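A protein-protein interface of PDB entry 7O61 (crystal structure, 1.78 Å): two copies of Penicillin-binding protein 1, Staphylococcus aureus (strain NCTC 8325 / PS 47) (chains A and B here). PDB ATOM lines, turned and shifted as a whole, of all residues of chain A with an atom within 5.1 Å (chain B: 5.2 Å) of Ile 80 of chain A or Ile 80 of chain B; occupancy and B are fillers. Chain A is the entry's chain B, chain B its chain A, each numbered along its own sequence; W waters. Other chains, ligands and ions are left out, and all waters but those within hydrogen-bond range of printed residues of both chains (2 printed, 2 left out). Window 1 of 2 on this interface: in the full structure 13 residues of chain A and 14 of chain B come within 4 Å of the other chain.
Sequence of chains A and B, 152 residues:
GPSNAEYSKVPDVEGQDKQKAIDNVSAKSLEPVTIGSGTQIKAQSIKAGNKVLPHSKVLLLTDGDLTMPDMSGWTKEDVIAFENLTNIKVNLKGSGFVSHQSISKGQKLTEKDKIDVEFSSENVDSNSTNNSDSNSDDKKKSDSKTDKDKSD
The side-chain amide nitrogen of Asn 84 of chain B lies within hydrogen-bond range of the backbone carbonyl oxygen of Ile 80 of chain B (3.5 Å).
Of the printed residues of chain B, Lys 76 of chain A touches Glu 83 (2.6 Å).
Glu 77 of chain A touches none of the printed residues of chain B.
Asp 78 of chain A touches none of the printed residues of chain B.
Of the printed residues of chain B, Ile 80 of chain A touches Lys 76 and Ile 80.
Printed residues of chain B within 4 Å of Glu 83 of chain A: Lys 76.
Of the printed residues of chain B, Leu 92 of chain A touches Leu 92 (2.9 Å).
Of the printed residues of chain A, Glu 77 of chain B touches Asn 84.
Printed residues of chain A within 4 Å of Ile 80 of chain B: Ile 80 (3.7 Å).
The nearest residue of chain B that does not touch Ile 80 of chain A is Glu 77 of chain B (4.2 Å).
Lys 76 of chain A touches Glu 83 of chain B, and with the chains exchanged Glu 83 of chain A touches Lys 76 of chain B.
Ile 80 of chain A touches Lys 76 of chain B, but with the chains exchanged Lys 76 of chain A does not touch Ile 80 of chain B (4.01 Å).
Ile 80 of chain A touches its own counterpart, Ile 80 of chain B.
Asn 84 of chain A touches Glu 77 of chain B, but with the chains exchanged Glu 77 of chain A does not touch Asn 84 of chain B (4.2 Å).
11 positions are printed for both chains.
Of the 6 pairs that touch across the chains among the printed residues, 4 have their exchanged pair printed and touching as well.
Water W2 bridges the backbone NH of Leu 92 of chain B (2.6 Å) and the backbone carbonyl oxygen of Leu 92 of chain A (2.9 Å).
Water W1 lies within hydrogen-bond range of the backbone carbonyl oxygen (O) of Leu 92 of chain B and the backbone NH (N) of Leu 92 of chain A.
The side-chain amino group of Lys 76 of chain B is in salt-bridge range of the side-chain carboxylate of Glu 83 of chain A (2.6 Å).
The side-chain carboxylate (OE1) of Glu 83 of chain B is in salt-bridge range of the side-chain amino group (NZ) of Lys 76 of chain A (2.6 Å).
O of Leu 92 of chain A lies close to O of Leu 92 of chain B.
Ile 80 of chain A touches Lys 76 of chain B.
Ile 80 of chain B touches Ile 80 of chain A.
Asn 84 of chain A touches Glu 77 of chain B (ND2 to OE2, 3.6 Å).
Of the 11 printed residues of chain B, 5 touch a printed residue of chain A.
Of the 11 printed residues of chain A, 5 touch a printed residue of chain B.
Hydrophobic or aromatic side chains of chain A within 4 Å of the printed part of chain B: Ile 80.
Along chain A the printed residues that touch a printed residue of chain B span positions 76 to 92.
Among the printed residues, 6 pairs touch across the chains.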
ATOM      1  N   LYS A  76     -10.437 -14.697  -9.923  1.00  0.00           N
ATOM      2  CA  LYS A  76     -11.611 -14.030 -10.475  1.00  0.00           C
ATOM      3  C   LYS A  76     -12.782 -14.106  -9.505  1.00  0.00           C
ATOM      4  O   LYS A  76     -13.514 -13.127  -9.320  1.00  0.00           O
ATOM      5  CB  LYS A  76     -11.986 -14.656 -11.815  1.00  0.00           C
ATOM      6  CG  LYS A  76     -11.024 -14.332 -12.931  1.00  0.00           C
ATOM      7  CD  LYS A  76     -11.714 -14.396 -14.286  1.00  0.00           C
ATOM      8  CE  LYS A  76     -10.700 -14.532 -15.405  1.00  0.00           C
ATOM      9  NZ  LYS A  76     -10.931 -15.733 -16.249  1.00  0.00           N
ATOM     10  N   GLU A  77     -12.957 -15.263  -8.861  1.00  0.00           N
ATOM     11  CA  GLU A  77     -14.021 -15.417  -7.876  1.00  0.00           C
ATOM     12  C   GLU A  77     -13.851 -14.456  -6.702  1.00  0.00           C
ATOM     13  O   GLU A  77     -14.840 -13.914  -6.194  1.00  0.00           O
ATOM     14  CB  GLU A  77     -14.064 -16.862  -7.389  1.00  0.00           C
ATOM     15  CG  GLU A  77     -15.384 -17.265  -6.791  1.00  0.00           C
ATOM     16  CD  GLU A  77     -15.379 -18.699  -6.320  1.00  0.00           C
ATOM     17  OE1 GLU A  77     -16.338 -19.426  -6.639  1.00  0.00           O
ATOM     18  OE2 GLU A  77     -14.413 -19.098  -5.636  1.00  0.00           O
ATOM     19  N   ASP A  78     -12.611 -14.240  -6.244  1.00  0.00           N
ATOM     20  CA  ASP A  78     -12.392 -13.259  -5.181  1.00  0.00           C
ATOM     21  C   ASP A  78     -12.813 -11.866  -5.624  1.00  0.00           C
ATOM     22  O   ASP A  78     -13.449 -11.126  -4.863  1.00  0.00           O
ATOM     23  CB  ASP A  78     -10.927 -13.215  -4.745  1.00  0.00           C
ATOM     24  CG  ASP A  78     -10.435 -14.518  -4.167  1.00  0.00           C
ATOM     25  OD1 ASP A  78     -11.187 -15.178  -3.411  1.00  0.00           O
ATOM     26  OD2 ASP A  78      -9.259 -14.844  -4.430  1.00  0.00           O
ATOM     27  N   VAL A  79     -12.444 -11.481  -6.847  1.00  0.00           N
ATOM     28  CA  VAL A  79     -12.709 -10.122  -7.298  1.00  0.00           C
ATOM     29  C   VAL A  79     -14.201  -9.911  -7.506  1.00  0.00           C
ATOM     30  O   VAL A  79     -14.740  -8.849  -7.172  1.00  0.00           O
ATOM     31  CB  VAL A  79     -11.900  -9.814  -8.572  1.00  0.00           C
ATOM     32  CG1 VAL A  79     -12.166  -8.400  -9.031  1.00  0.00           C
ATOM     33  CG2 VAL A  79     -10.415  -9.995  -8.312  1.00  0.00           C
ATOM     34  N   ILE A  80     -14.901 -10.917  -8.042  1.00  0.00           N
ATOM     35  CA  ILE A  80     -16.337 -10.749  -8.226  1.00  0.00           C
ATOM     36  C   ILE A  80     -17.040 -10.729  -6.876  1.00  0.00           C
ATOM     37  O   ILE A  80     -18.037 -10.016  -6.699  1.00  0.00           O
ATOM     38  CB  ILE A  80     -16.913 -11.826  -9.170  1.00  0.00           C
ATOM     39  CG1 ILE A  80     -18.369 -11.508  -9.499  1.00  0.00           C
ATOM     40  CG2 ILE A  80     -16.830 -13.211  -8.553  1.00  0.00           C
ATOM     41  CD1 ILE A  80     -18.527 -10.328 -10.425  1.00  0.00           C
ATOM     42  N   ALA A  81     -16.520 -11.474  -5.895  1.00  0.00           N
ATOM     43  CA  ALA A  81     -17.036 -11.361  -4.536  1.00  0.00           C
ATOM     44  C   ALA A  81     -16.941  -9.924  -4.041  1.00  0.00           C
ATOM     45  O   ALA A  81     -17.886  -9.403  -3.437  1.00  0.00           O
ATOM     46  CB  ALA A  81     -16.272 -12.302  -3.603  1.00  0.00           C
ATOM     47  N   PHE A  82     -15.806  -9.268  -4.297  1.00  0.00           N
ATOM     48  CA  PHE A  82     -15.653  -7.859  -3.954  1.00  0.00           C
ATOM     49  C   PHE A  82     -16.712  -7.005  -4.642  1.00  0.00           C
ATOM     50  O   PHE A  82     -17.330  -6.137  -4.013  1.00  0.00           O
ATOM     51  CB  PHE A  82     -14.247  -7.392  -4.333  1.00  0.00           C
ATOM     52  CG  PHE A  82     -14.009  -5.931  -4.107  1.00  0.00           C
ATOM     53  CD1 PHE A  82     -14.265  -5.006  -5.106  1.00  0.00           C
ATOM     54  CD2 PHE A  82     -13.521  -5.481  -2.896  1.00  0.00           C
ATOM     55  CE1 PHE A  82     -14.042  -3.660  -4.894  1.00  0.00           C
ATOM     56  CE2 PHE A  82     -13.300  -4.138  -2.680  1.00  0.00           C
ATOM     57  CZ  PHE A  82     -13.556  -3.229  -3.677  1.00  0.00           C
ATOM     58  N   GLU A  83     -16.916  -7.225  -5.946  1.00  0.00           N
ATOM     59  CA  GLU A  83     -17.930  -6.480  -6.687  1.00  0.00           C
ATOM     60  C   GLU A  83     -19.302  -6.639  -6.051  1.00  0.00           C
ATOM     61  O   GLU A  83     -20.024  -5.657  -5.842  1.00  0.00           O
ATOM     62  CB  GLU A  83     -17.969  -6.946  -8.146  1.00  0.00           C
ATOM     63  CG  GLU A  83     -18.701  -5.990  -9.075  1.00  0.00           C
ATOM     64  CD  GLU A  83     -18.778  -6.492 -10.504  1.00  0.00           C
ATOM     65  OE1 GLU A  83     -19.783  -7.146 -10.861  1.00  0.00           O
ATOM     66  OE2 GLU A  83     -17.830  -6.236 -11.271  1.00  0.00           O
ATOM     67  N   ASN A  84     -19.681  -7.877  -5.737  1.00  0.00           N
ATOM     68  CA  ASN A  84     -21.018  -8.107  -5.208  1.00  0.00           C
ATOM     69  C   ASN A  84     -21.148  -7.571  -3.791  1.00  0.00           C
ATOM     70  O   ASN A  84     -22.231  -7.131  -3.390  1.00  0.00           O
ATOM     71  CB  ASN A  84     -21.344  -9.599  -5.270  1.00  0.00           C
ATOM     72  CG  ASN A  84     -21.560 -10.088  -6.695  1.00  0.00           C
ATOM     73  OD1 ASN A  84     -21.944  -9.317  -7.577  1.00  0.00           O
ATOM     74  ND2 ASN A  84     -21.293 -11.368  -6.930  1.00  0.00           N
ATOM     75  N   LEU A  85     -20.050  -7.563  -3.034  1.00  0.00           N
ATOM     76  CA  LEU A  85     -20.104  -7.102  -1.654  1.00  0.00           C
ATOM     77  C   LEU A  85     -20.206  -5.584  -1.581  1.00  0.00           C
ATOM     78  O   LEU A  85     -20.909  -5.044  -0.720  1.00  0.00           O
ATOM     79  CB  LEU A  85     -18.868  -7.595  -0.902  1.00  0.00           C
ATOM     80  CG  LEU A  85     -18.751  -7.306   0.589  1.00  0.00           C
ATOM     81  CD1 LEU A  85     -19.850  -8.023   1.359  1.00  0.00           C
ATOM     82  CD2 LEU A  85     -17.384  -7.742   1.076  1.00  0.00           C
ATOM     83  N   LEU A  92     -12.381  -7.215 -15.302  1.00  0.00           N
ATOM     84  CA  LEU A  92     -11.378  -8.264 -15.212  1.00  0.00           C
ATOM     85  C   LEU A  92     -10.721  -8.426 -16.576  1.00  0.00           C
ATOM     86  O   LEU A  92     -11.420  -8.666 -17.565  1.00  0.00           O
ATOM     87  CB  LEU A  92     -12.039  -9.588 -14.807  1.00  0.00           C
ATOM     88  CG  LEU A  92     -13.149  -9.553 -13.754  1.00  0.00           C
ATOM     89  CD1 LEU A  92     -13.568 -10.955 -13.344  1.00  0.00           C
ATOM     90  CD2 LEU A  92     -12.732  -8.778 -12.535  1.00  0.00           C
ATOM     91  N   LYS B  76     -21.675 -12.145 -14.240  1.00  0.00           N
ATOM     92  CA  LYS B  76     -20.255 -12.478 -14.211  1.00  0.00           C
ATOM     93  C   LYS B  76     -19.994 -13.665 -13.295  1.00  0.00           C
ATOM     94  O   LYS B  76     -19.186 -14.542 -13.618  1.00  0.00           O
ATOM     95  CB  LYS B  76     -19.434 -11.259 -13.773  1.00  0.00           C
ATOM     96  CG  LYS B  76     -19.437 -10.137 -14.790  1.00  0.00           C
ATOM     97  CD  LYS B  76     -18.270  -9.196 -14.603  1.00  0.00           C
ATOM     98  CE  LYS B  76     -18.729  -7.907 -13.964  1.00  0.00           C
ATOM     99  NZ  LYS B  76     -17.591  -6.995 -13.737  1.00  0.00           N
ATOM    100  N   GLU B  77     -20.691 -13.719 -12.155  1.00  0.00           N
ATOM    101  CA  GLU B  77     -20.563 -14.850 -11.243  1.00  0.00           C
ATOM    102  C   GLU B  77     -20.919 -16.169 -11.922  1.00  0.00           C
ATOM    103  O   GLU B  77     -20.259 -17.190 -11.687  1.00  0.00           O
ATOM    104  CB  GLU B  77     -21.450 -14.626 -10.018  1.00  0.00           C
ATOM    105  CG  GLU B  77     -21.170 -15.565  -8.866  1.00  0.00           C
ATOM    106  CD  GLU B  77     -21.945 -15.190  -7.619  1.00  0.00           C
ATOM    107  OE1 GLU B  77     -21.550 -15.622  -6.516  1.00  0.00           O
ATOM    108  OE2 GLU B  77     -22.949 -14.455  -7.742  1.00  0.00           O
ATOM    109  N   ASP B  78     -21.971 -16.174 -12.753  1.00  0.00           N
ATOM    110  CA  ASP B  78     -22.327 -17.391 -13.484  1.00  0.00           C
ATOM    111  C   ASP B  78     -21.206 -17.814 -14.419  1.00  0.00           C
ATOM    112  O   ASP B  78     -20.873 -19.001 -14.513  1.00  0.00           O
ATOM    113  CB  ASP B  78     -23.606 -17.198 -14.302  1.00  0.00           C
ATOM    114  CG  ASP B  78     -24.811 -16.862 -13.455  1.00  0.00           C
ATOM    115  OD1 ASP B  78     -24.971 -17.465 -12.377  1.00  0.00           O
ATOM    116  OD2 ASP B  78     -25.635 -16.035 -13.903  1.00  0.00           O
ATOM    117  N   VAL B  79     -20.629 -16.851 -15.136  1.00  0.00           N
ATOM    118  CA  VAL B  79     -19.606 -17.164 -16.123  1.00  0.00           C
ATOM    119  C   VAL B  79     -18.338 -17.659 -15.440  1.00  0.00           C
ATOM    120  O   VAL B  79     -17.688 -18.596 -15.915  1.00  0.00           O
ATOM    121  CB  VAL B  79     -19.344 -15.931 -17.007  1.00  0.00           C
ATOM    122  CG1 VAL B  79     -18.196 -16.188 -17.953  1.00  0.00           C
ATOM    123  CG2 VAL B  79     -20.604 -15.556 -17.778  1.00  0.00           C
ATOM    124  N   ILE B  80     -17.965 -17.044 -14.314  1.00  0.00           N
ATOM    125  CA  ILE B  80     -16.803 -17.521 -13.569  1.00  0.00           C
ATOM    126  C   ILE B  80     -17.044 -18.928 -13.037  1.00  0.00           C
ATOM    127  O   ILE B  80     -16.137 -19.768 -13.039  1.00  0.00           O
ATOM    128  CB  ILE B  80     -16.423 -16.525 -12.453  1.00  0.00           C
ATOM    129  CG1 ILE B  80     -16.171 -15.130 -13.048  1.00  0.00           C
ATOM    130  CG2 ILE B  80     -15.223 -17.023 -11.659  1.00  0.00           C
ATOM    131  CD1 ILE B  80     -16.527 -13.971 -12.127  1.00  0.00           C
ATOM    132  N   ALA B  81     -18.270 -19.215 -12.588  1.00  0.00           N
ATOM    133  CA  ALA B  81     -18.610 -20.581 -12.199  1.00  0.00           C
ATOM    134  C   ALA B  81     -18.392 -21.554 -13.354  1.00  0.00           C
ATOM    135  O   ALA B  81     -17.917 -22.678 -13.151  1.00  0.00           O
ATOM    136  CB  ALA B  81     -20.057 -20.646 -11.711  1.00  0.00           C
ATOM    137  N   PHE B  82     -18.731 -21.140 -14.575  1.00  0.00           N
ATOM    138  CA  PHE B  82     -18.502 -22.012 -15.721  1.00  0.00           C
ATOM    139  C   PHE B  82     -17.013 -22.261 -15.923  1.00  0.00           C
ATOM    140  O   PHE B  82     -16.596 -23.395 -16.185  1.00  0.00           O
ATOM    141  CB  PHE B  82     -19.127 -21.405 -16.978  1.00  0.00           C
ATOM    142  CG  PHE B  82     -18.747 -22.112 -18.248  1.00  0.00           C
ATOM    143  CD1 PHE B  82     -17.616 -21.741 -18.960  1.00  0.00           C
ATOM    144  CD2 PHE B  82     -19.527 -23.152 -18.728  1.00  0.00           C
ATOM    145  CE1 PHE B  82     -17.270 -22.398 -20.130  1.00  0.00           C
ATOM    146  CE2 PHE B  82     -19.186 -23.807 -19.894  1.00  0.00           C
ATOM    147  CZ  PHE B  82     -18.066 -23.434 -20.595  1.00  0.00           C
ATOM    148  N   GLU B  83     -16.195 -21.211 -15.806  1.00  0.00           N
ATOM    149  CA  GLU B  83     -14.757 -21.382 -15.983  1.00  0.00           C
ATOM    150  C   GLU B  83     -14.200 -22.361 -14.961  1.00  0.00           C
ATOM    151  O   GLU B  83     -13.391 -23.233 -15.299  1.00  0.00           O
ATOM    152  CB  GLU B  83     -14.035 -20.032 -15.868  1.00  0.00           C
ATOM    153  CG  GLU B  83     -12.528 -20.177 -15.714  1.00  0.00           C
ATOM    154  CD  GLU B  83     -11.760 -18.861 -15.859  1.00  0.00           C
ATOM    155  OE1 GLU B  83     -12.174 -17.984 -16.645  1.00  0.00           O
ATOM    156  OE2 GLU B  83     -10.730 -18.708 -15.172  1.00  0.00           O
ATOM    157  N   ASN B  84     -14.630 -22.238 -13.703  1.00  0.00           N
ATOM    158  CA  ASN B  84     -14.101 -23.107 -12.662  1.00  0.00           C
ATOM    159  C   ASN B  84     -14.609 -24.531 -12.821  1.00  0.00           C
ATOM    160  O   ASN B  84     -13.898 -25.482 -12.482  1.00  0.00           O
ATOM    161  CB  ASN B  84     -14.470 -22.559 -11.284  1.00  0.00           C
ATOM    162  CG  ASN B  84     -13.700 -21.300 -10.936  1.00  0.00           C
ATOM    163  OD1 ASN B  84     -12.561 -21.124 -11.365  1.00  0.00           O
ATOM    164  ND2 ASN B  84     -14.316 -20.420 -10.155  1.00  0.00           N
ATOM    165  N   LEU B  85     -15.822 -24.696 -13.347  1.00  0.00           N
ATOM    166  CA  LEU B  85     -16.395 -26.030 -13.466  1.00  0.00           C
ATOM    167  C   LEU B  85     -15.758 -26.804 -14.613  1.00  0.00           C
ATOM    168  O   LEU B  85     -15.523 -28.011 -14.496  1.00  0.00           O
ATOM    169  CB  LEU B  85     -17.908 -25.919 -13.654  1.00  0.00           C
ATOM    170  CG  LEU B  85     -18.743 -27.194 -13.578  1.00  0.00           C
ATOM    171  CD1 LEU B  85     -18.614 -27.841 -12.211  1.00  0.00           C
ATOM    172  CD2 LEU B  85     -20.195 -26.862 -13.886  1.00  0.00           C
ATOM    173  N   LEU B  92     -13.639 -12.084 -19.696  1.00  0.00           N
ATOM    174  CA  LEU B  92     -14.847 -11.327 -19.397  1.00  0.00           C
ATOM    175  C   LEU B  92     -14.617  -9.866 -19.756  1.00  0.00           C
ATOM    176  O   LEU B  92     -13.705  -9.228 -19.220  1.00  0.00           O
ATOM    177  CB  LEU B  92     -15.222 -11.470 -17.920  1.00  0.00           C
ATOM    178  CG  LEU B  92     -15.703 -12.850 -17.464  1.00  0.00           C
ATOM    179  CD1 LEU B  92     -14.532 -13.739 -17.072  1.00  0.00           C
ATOM    180  CD2 LEU B  92     -16.671 -12.707 -16.301  1.00  0.00           C
HETATM  181  O   HOH W   1     -14.902  -7.744 -16.888  1.00  0.00           O
HETATM  182  O   HOH W   2     -11.834 -11.508 -17.856  1.00  0.00           O
